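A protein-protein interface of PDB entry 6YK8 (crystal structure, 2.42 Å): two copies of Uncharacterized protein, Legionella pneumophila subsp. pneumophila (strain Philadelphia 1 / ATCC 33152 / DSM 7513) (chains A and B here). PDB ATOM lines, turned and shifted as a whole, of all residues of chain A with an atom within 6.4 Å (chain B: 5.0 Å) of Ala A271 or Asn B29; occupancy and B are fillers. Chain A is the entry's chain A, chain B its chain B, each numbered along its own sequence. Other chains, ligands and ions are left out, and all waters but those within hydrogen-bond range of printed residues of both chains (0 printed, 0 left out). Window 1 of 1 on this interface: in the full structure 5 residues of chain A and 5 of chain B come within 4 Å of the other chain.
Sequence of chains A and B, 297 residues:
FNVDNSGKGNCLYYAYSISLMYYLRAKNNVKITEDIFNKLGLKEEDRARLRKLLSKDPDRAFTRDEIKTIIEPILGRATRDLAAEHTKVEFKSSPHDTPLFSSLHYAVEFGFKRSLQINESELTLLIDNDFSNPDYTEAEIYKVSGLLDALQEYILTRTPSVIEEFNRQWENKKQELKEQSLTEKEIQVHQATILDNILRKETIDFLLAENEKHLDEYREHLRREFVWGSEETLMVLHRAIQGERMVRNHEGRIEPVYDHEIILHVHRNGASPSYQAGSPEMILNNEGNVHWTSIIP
The backbone carbonyl oxygen (O) of Ser A272 lies within hydrogen-bond range of the backbone NH (N) of Val B30 (3.3 Å).
O of Asn B29 lies within hydrogen-bond range of OG1 of Thr B33, 2.9 Å away.
The side-chain amide oxygen (OD1) of Asn B29 is in hydrogen-bond range of the backbone NH (N) of Ile B32 (3.1 Å).
ND2 of Asn B29 touches CB of Ala A271, 3.2 Å away.
Ser A272 touches Asn B28 (O to O, 3.8 Å).
O of Ser A272 touches CA of Asn B29, 3.8 Å away.
OD1 of Asn B28 touches CB of Pro A273 (3.3 Å).
Of chain B, only Asn B29 (3.2 Å) comes within 4 Å of Ala A271.
Printed residues of chain B within 4 Å of Ser A272: Asn B28 (3.8 Å), Asn B29 (3.8 Å) and Val B30 (3.3 Å).
Printed residues of chain B within 4 Å of Pro A273: Asn B28.
Of the printed residues of chain A, Asn B28 touches Ser A272 (3.8 Å) and Pro A273 (3.3 Å).
Asn B29 touches just these residues of chain A: Ala A271 and Ser A272.
Printed residues of chain A within 4 Å of Val B30: Ser A272 (3.3 Å).
Ile B32 touches none of the printed residues of chain A.
The nearest printed residue of chain B that does not touch Ala A271 is Asn B28 (5.3 Å).
The nearest printed residue of chain B that does not touch Ser A272 is Lys B31 (5.4 Å).
Of the 9 printed residues of chain A, 3 touch a printed residue of chain B.
Printed residues of chain A that touch a printed residue of chain B: Ala A271, Ser A272 and Pro A273.
Of the 8 printed residues of chain B, 3 touch a printed residue of chain A.
Printed residues of chain B that touch a printed residue of chain A: Asn B28, Asn B29 and Val B30.
Hydrophobic or aromatic side chains of chain B that line the printed part of chain A: Val B30.
No position is printed for both chains.
Of the 5 pairs that touch across the chains among the printed residues, none has its exchanged pair printed and touching as well.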
ATOM      1  N   VAL A 266      25.089  20.835  10.678  1.00  0.00           N
ATOM      2  CA  VAL A 266      26.140  19.844  10.558  1.00  0.00           C
ATOM      3  C   VAL A 266      26.094  19.274   9.153  1.00  0.00           C
ATOM      4  O   VAL A 266      25.017  19.035   8.587  1.00  0.00           O
ATOM      5  CB  VAL A 266      26.012  18.743  11.624  1.00  0.00           C
ATOM      6  CG1 VAL A 266      27.247  17.879  11.615  1.00  0.00           C
ATOM      7  CG2 VAL A 266      25.862  19.375  12.981  1.00  0.00           C
ATOM      8  N   HIS A 267      27.271  19.122   8.567  1.00  0.00           N
ATOM      9  CA  HIS A 267      27.470  18.423   7.316  1.00  0.00           C
ATOM     10  C   HIS A 267      28.198  17.121   7.625  1.00  0.00           C
ATOM     11  O   HIS A 267      28.932  17.026   8.616  1.00  0.00           O
ATOM     12  CB  HIS A 267      28.257  19.298   6.329  1.00  0.00           C
ATOM     13  CG  HIS A 267      27.488  20.497   5.860  1.00  0.00           C
ATOM     14  ND1 HIS A 267      28.053  21.509   5.114  1.00  0.00           N
ATOM     15  CD2 HIS A 267      26.196  20.854   6.059  1.00  0.00           C
ATOM     16  CE1 HIS A 267      27.137  22.427   4.854  1.00  0.00           C
ATOM     17  NE2 HIS A 267      26.001  22.053   5.417  1.00  0.00           N
ATOM     18  N   ARG A 268      27.954  16.098   6.806  1.00  0.00           N
ATOM     19  CA  ARG A 268      28.513  14.770   7.055  1.00  0.00           C
ATOM     20  C   ARG A 268      29.133  14.235   5.769  1.00  0.00           C
ATOM     21  O   ARG A 268      28.419  13.927   4.808  1.00  0.00           O
ATOM     22  CB  ARG A 268      27.456  13.814   7.617  1.00  0.00           C
ATOM     23  CG  ARG A 268      27.495  13.691   9.155  1.00  0.00           C
ATOM     24  CD  ARG A 268      27.067  12.293   9.642  1.00  0.00           C
ATOM     25  NE  ARG A 268      28.191  11.358   9.763  1.00  0.00           N
ATOM     26  CZ  ARG A 268      28.073  10.031   9.720  1.00  0.00           C
ATOM     27  NH1 ARG A 268      29.151   9.259   9.829  1.00  0.00           N
ATOM     28  NH2 ARG A 268      26.881   9.474   9.549  1.00  0.00           N
ATOM     29  N   ASN A 269      30.468  14.136   5.770  1.00  0.00           N
ATOM     30  CA  ASN A 269      31.263  13.718   4.614  1.00  0.00           C
ATOM     31  C   ASN A 269      30.999  14.616   3.407  1.00  0.00           C
ATOM     32  O   ASN A 269      30.990  14.154   2.260  1.00  0.00           O
ATOM     33  CB  ASN A 269      31.019  12.240   4.278  1.00  0.00           C
ATOM     34  CG  ASN A 269      31.394  11.297   5.439  1.00  0.00           C
ATOM     35  OD1 ASN A 269      30.553  10.947   6.273  1.00  0.00           O
ATOM     36  ND2 ASN A 269      32.660  10.884   5.484  1.00  0.00           N
ATOM     37  N   GLY A 270      30.776  15.911   3.668  1.00  0.00           N
ATOM     38  CA  GLY A 270      30.534  16.899   2.647  1.00  0.00           C
ATOM     39  C   GLY A 270      29.072  17.182   2.359  1.00  0.00           C
ATOM     40  O   GLY A 270      28.765  18.250   1.816  1.00  0.00           O
ATOM     41  N   ALA A 271      28.166  16.262   2.698  1.00  0.00           N
ATOM     42  CA  ALA A 271      26.748  16.458   2.416  1.00  0.00           C
ATOM     43  C   ALA A 271      26.244  17.736   3.087  1.00  0.00           C
ATOM     44  O   ALA A 271      26.897  18.290   3.959  1.00  0.00           O
ATOM     45  CB  ALA A 271      25.945  15.253   2.904  1.00  0.00           C
ATOM     46  N   SER A 272      25.072  18.212   2.678  1.00  0.00           N
ATOM     47  CA  SER A 272      24.439  19.349   3.334  1.00  0.00           C
ATOM     48  C   SER A 272      22.960  19.081   3.594  1.00  0.00           C
ATOM     49  O   SER A 272      22.335  18.261   2.912  1.00  0.00           O
ATOM     50  CB  SER A 272      24.594  20.639   2.511  1.00  0.00           C
ATOM     51  OG  SER A 272      24.554  20.371   1.118  1.00  0.00           O
ATOM     52  N   PRO A 273      22.370  19.757   4.597  1.00  0.00           N
ATOM     53  CA  PRO A 273      20.956  19.484   4.863  1.00  0.00           C
ATOM     54  C   PRO A 273      20.050  20.112   3.810  1.00  0.00           C
ATOM     55  O   PRO A 273      19.052  19.486   3.452  1.00  0.00           O
ATOM     56  CB  PRO A 273      20.727  20.122   6.245  1.00  0.00           C
ATOM     57  CG  PRO A 273      22.108  20.325   6.822  1.00  0.00           C
ATOM     58  CD  PRO A 273      22.951  20.636   5.623  1.00  0.00           C
ATOM     59  N   ASN A 285      31.425  20.339   9.395  1.00  0.00           N
ATOM     60  CA  ASN A 285      31.397  19.084   8.679  1.00  0.00           C
ATOM     61  C   ASN A 285      31.875  17.986   9.616  1.00  0.00           C
ATOM     62  O   ASN A 285      32.914  18.136  10.271  1.00  0.00           O
ATOM     63  CB  ASN A 285      32.265  19.116   7.424  1.00  0.00           C
ATOM     64  CG  ASN A 285      32.305  17.761   6.742  1.00  0.00           C
ATOM     65  OD1 ASN A 285      31.295  17.308   6.224  1.00  0.00           O
ATOM     66  ND2 ASN A 285      33.452  17.094   6.782  1.00  0.00           N
ATOM     67  N   LYS B  27      18.954  11.503   8.889  1.00  0.00           N
ATOM     68  CA  LYS B  27      20.300  11.646   8.340  1.00  0.00           C
ATOM     69  C   LYS B  27      20.544  13.032   7.747  1.00  0.00           C
ATOM     70  O   LYS B  27      21.680  13.519   7.777  1.00  0.00           O
ATOM     71  CB  LYS B  27      20.553  10.577   7.266  1.00  0.00           C
ATOM     72  CG  LYS B  27      21.262   9.331   7.771  1.00  0.00           C
ATOM     73  CD  LYS B  27      22.213   8.796   6.715  1.00  0.00           C
ATOM     74  CE  LYS B  27      23.577   8.410   7.295  1.00  0.00           C
ATOM     75  NZ  LYS B  27      24.591   8.248   6.195  1.00  0.00           N
ATOM     76  N   ASN B  28      19.514  13.663   7.183  1.00  0.00           N
ATOM     77  CA  ASN B  28      19.577  15.055   6.737  1.00  0.00           C
ATOM     78  C   ASN B  28      20.674  15.256   5.686  1.00  0.00           C
ATOM     79  O   ASN B  28      21.615  16.032   5.868  1.00  0.00           O
ATOM     80  CB  ASN B  28      19.770  15.999   7.933  1.00  0.00           C
ATOM     81  CG  ASN B  28      19.032  17.309   7.761  1.00  0.00           C
ATOM     82  OD1 ASN B  28      18.581  17.633   6.665  1.00  0.00           O
ATOM     83  ND2 ASN B  28      18.916  18.079   8.842  1.00  0.00           N
ATOM     84  N   ASN B  29      20.537  14.518   4.584  1.00  0.00           N
ATOM     85  CA  ASN B  29      21.384  14.656   3.407  1.00  0.00           C
ATOM     86  C   ASN B  29      20.464  14.765   2.206  1.00  0.00           C
ATOM     87  O   ASN B  29      19.642  13.873   1.959  1.00  0.00           O
ATOM     88  CB  ASN B  29      22.352  13.473   3.248  1.00  0.00           C
ATOM     89  CG  ASN B  29      23.117  13.490   1.903  1.00  0.00           C
ATOM     90  OD1 ASN B  29      22.732  14.160   0.939  1.00  0.00           O
ATOM     91  ND2 ASN B  29      24.213  12.736   1.848  1.00  0.00           N
ATOM     92  N   VAL B  30      20.623  15.845   1.448  1.00  0.00           N
ATOM     93  CA  VAL B  30      19.779  16.033   0.280  1.00  0.00           C
ATOM     94  C   VAL B  30      20.015  14.917  -0.717  1.00  0.00           C
ATOM     95  O   VAL B  30      19.076  14.433  -1.351  1.00  0.00           O
ATOM     96  CB  VAL B  30      20.025  17.413  -0.353  1.00  0.00           C
ATOM     97  CG1 VAL B  30      21.514  17.618  -0.578  1.00  0.00           C
ATOM     98  CG2 VAL B  30      19.243  17.544  -1.660  1.00  0.00           C
ATOM     99  N   LYS B  31      21.262  14.466  -0.848  1.00  0.00           N
ATOM    100  CA  LYS B  31      21.622  13.554  -1.925  1.00  0.00           C
ATOM    101  C   LYS B  31      21.259  12.109  -1.644  1.00  0.00           C
ATOM    102  O   LYS B  31      20.769  11.404  -2.539  1.00  0.00           O
ATOM    103  CB  LYS B  31      23.113  13.671  -2.235  1.00  0.00           C
ATOM    104  CG  LYS B  31      23.291  14.914  -3.021  1.00  0.00           C
ATOM    105  CD  LYS B  31      22.650  14.583  -4.390  1.00  0.00           C
ATOM    106  CE  LYS B  31      22.070  15.782  -5.172  1.00  0.00           C
ATOM    107  NZ  LYS B  31      20.891  15.556  -5.900  1.00  0.00           N
ATOM    108  N   ILE B  32      21.526  11.653  -0.425  1.00  0.00           N
ATOM    109  CA  ILE B  32      20.998  10.370   0.011  1.00  0.00           C
ATOM    110  C   ILE B  32      19.497  10.344  -0.228  1.00  0.00           C
ATOM    111  O   ILE B  32      18.961   9.415  -0.849  1.00  0.00           O
ATOM    112  CB  ILE B  32      21.352  10.139   1.486  1.00  0.00           C
ATOM    113  CG1 ILE B  32      22.788   9.632   1.608  1.00  0.00           C
ATOM    114  CG2 ILE B  32      20.370   9.209   2.105  1.00  0.00           C
ATOM    115  CD1 ILE B  32      23.133   9.181   3.011  1.00  0.00           C
ATOM    116  N   THR B  33      18.815  11.421   0.180  1.00  0.00           N
ATOM    117  CA  THR B  33      17.387  11.546  -0.088  1.00  0.00           C
ATOM    118  C   THR B  33      17.102  11.499  -1.573  1.00  0.00           C
ATOM    119  O   THR B  33      16.195  10.794  -2.025  1.00  0.00           O
ATOM    120  CB  THR B  33      16.837  12.848   0.478  1.00  0.00           C
ATOM    121  OG1 THR B  33      16.927  12.826   1.900  1.00  0.00           O
ATOM    122  CG2 THR B  33      15.378  13.021   0.032  1.00  0.00           C
ATOM    123  N   GLU B  34      17.855  12.258  -2.351  1.00  0.00           N
ATOM    124  CA  GLU B  34      17.498  12.369  -3.753  1.00  0.00           C
ATOM    125  C   GLU B  34      17.882  11.113  -4.509  1.00  0.00           C
ATOM    126  O   GLU B  34      17.165  10.697  -5.422  1.00  0.00           O
ATOM    127  CB  GLU B  34      18.147  13.597  -4.368  1.00  0.00           C
ATOM    128  CG  GLU B  34      17.565  14.928  -3.904  1.00  0.00           C
ATOM    129  CD  GLU B  34      16.082  15.056  -4.174  1.00  0.00           C
ATOM    130  OE1 GLU B  34      15.344  15.432  -3.244  1.00  0.00           O
ATOM    131  OE2 GLU B  34      15.658  14.790  -5.318  1.00  0.00           O
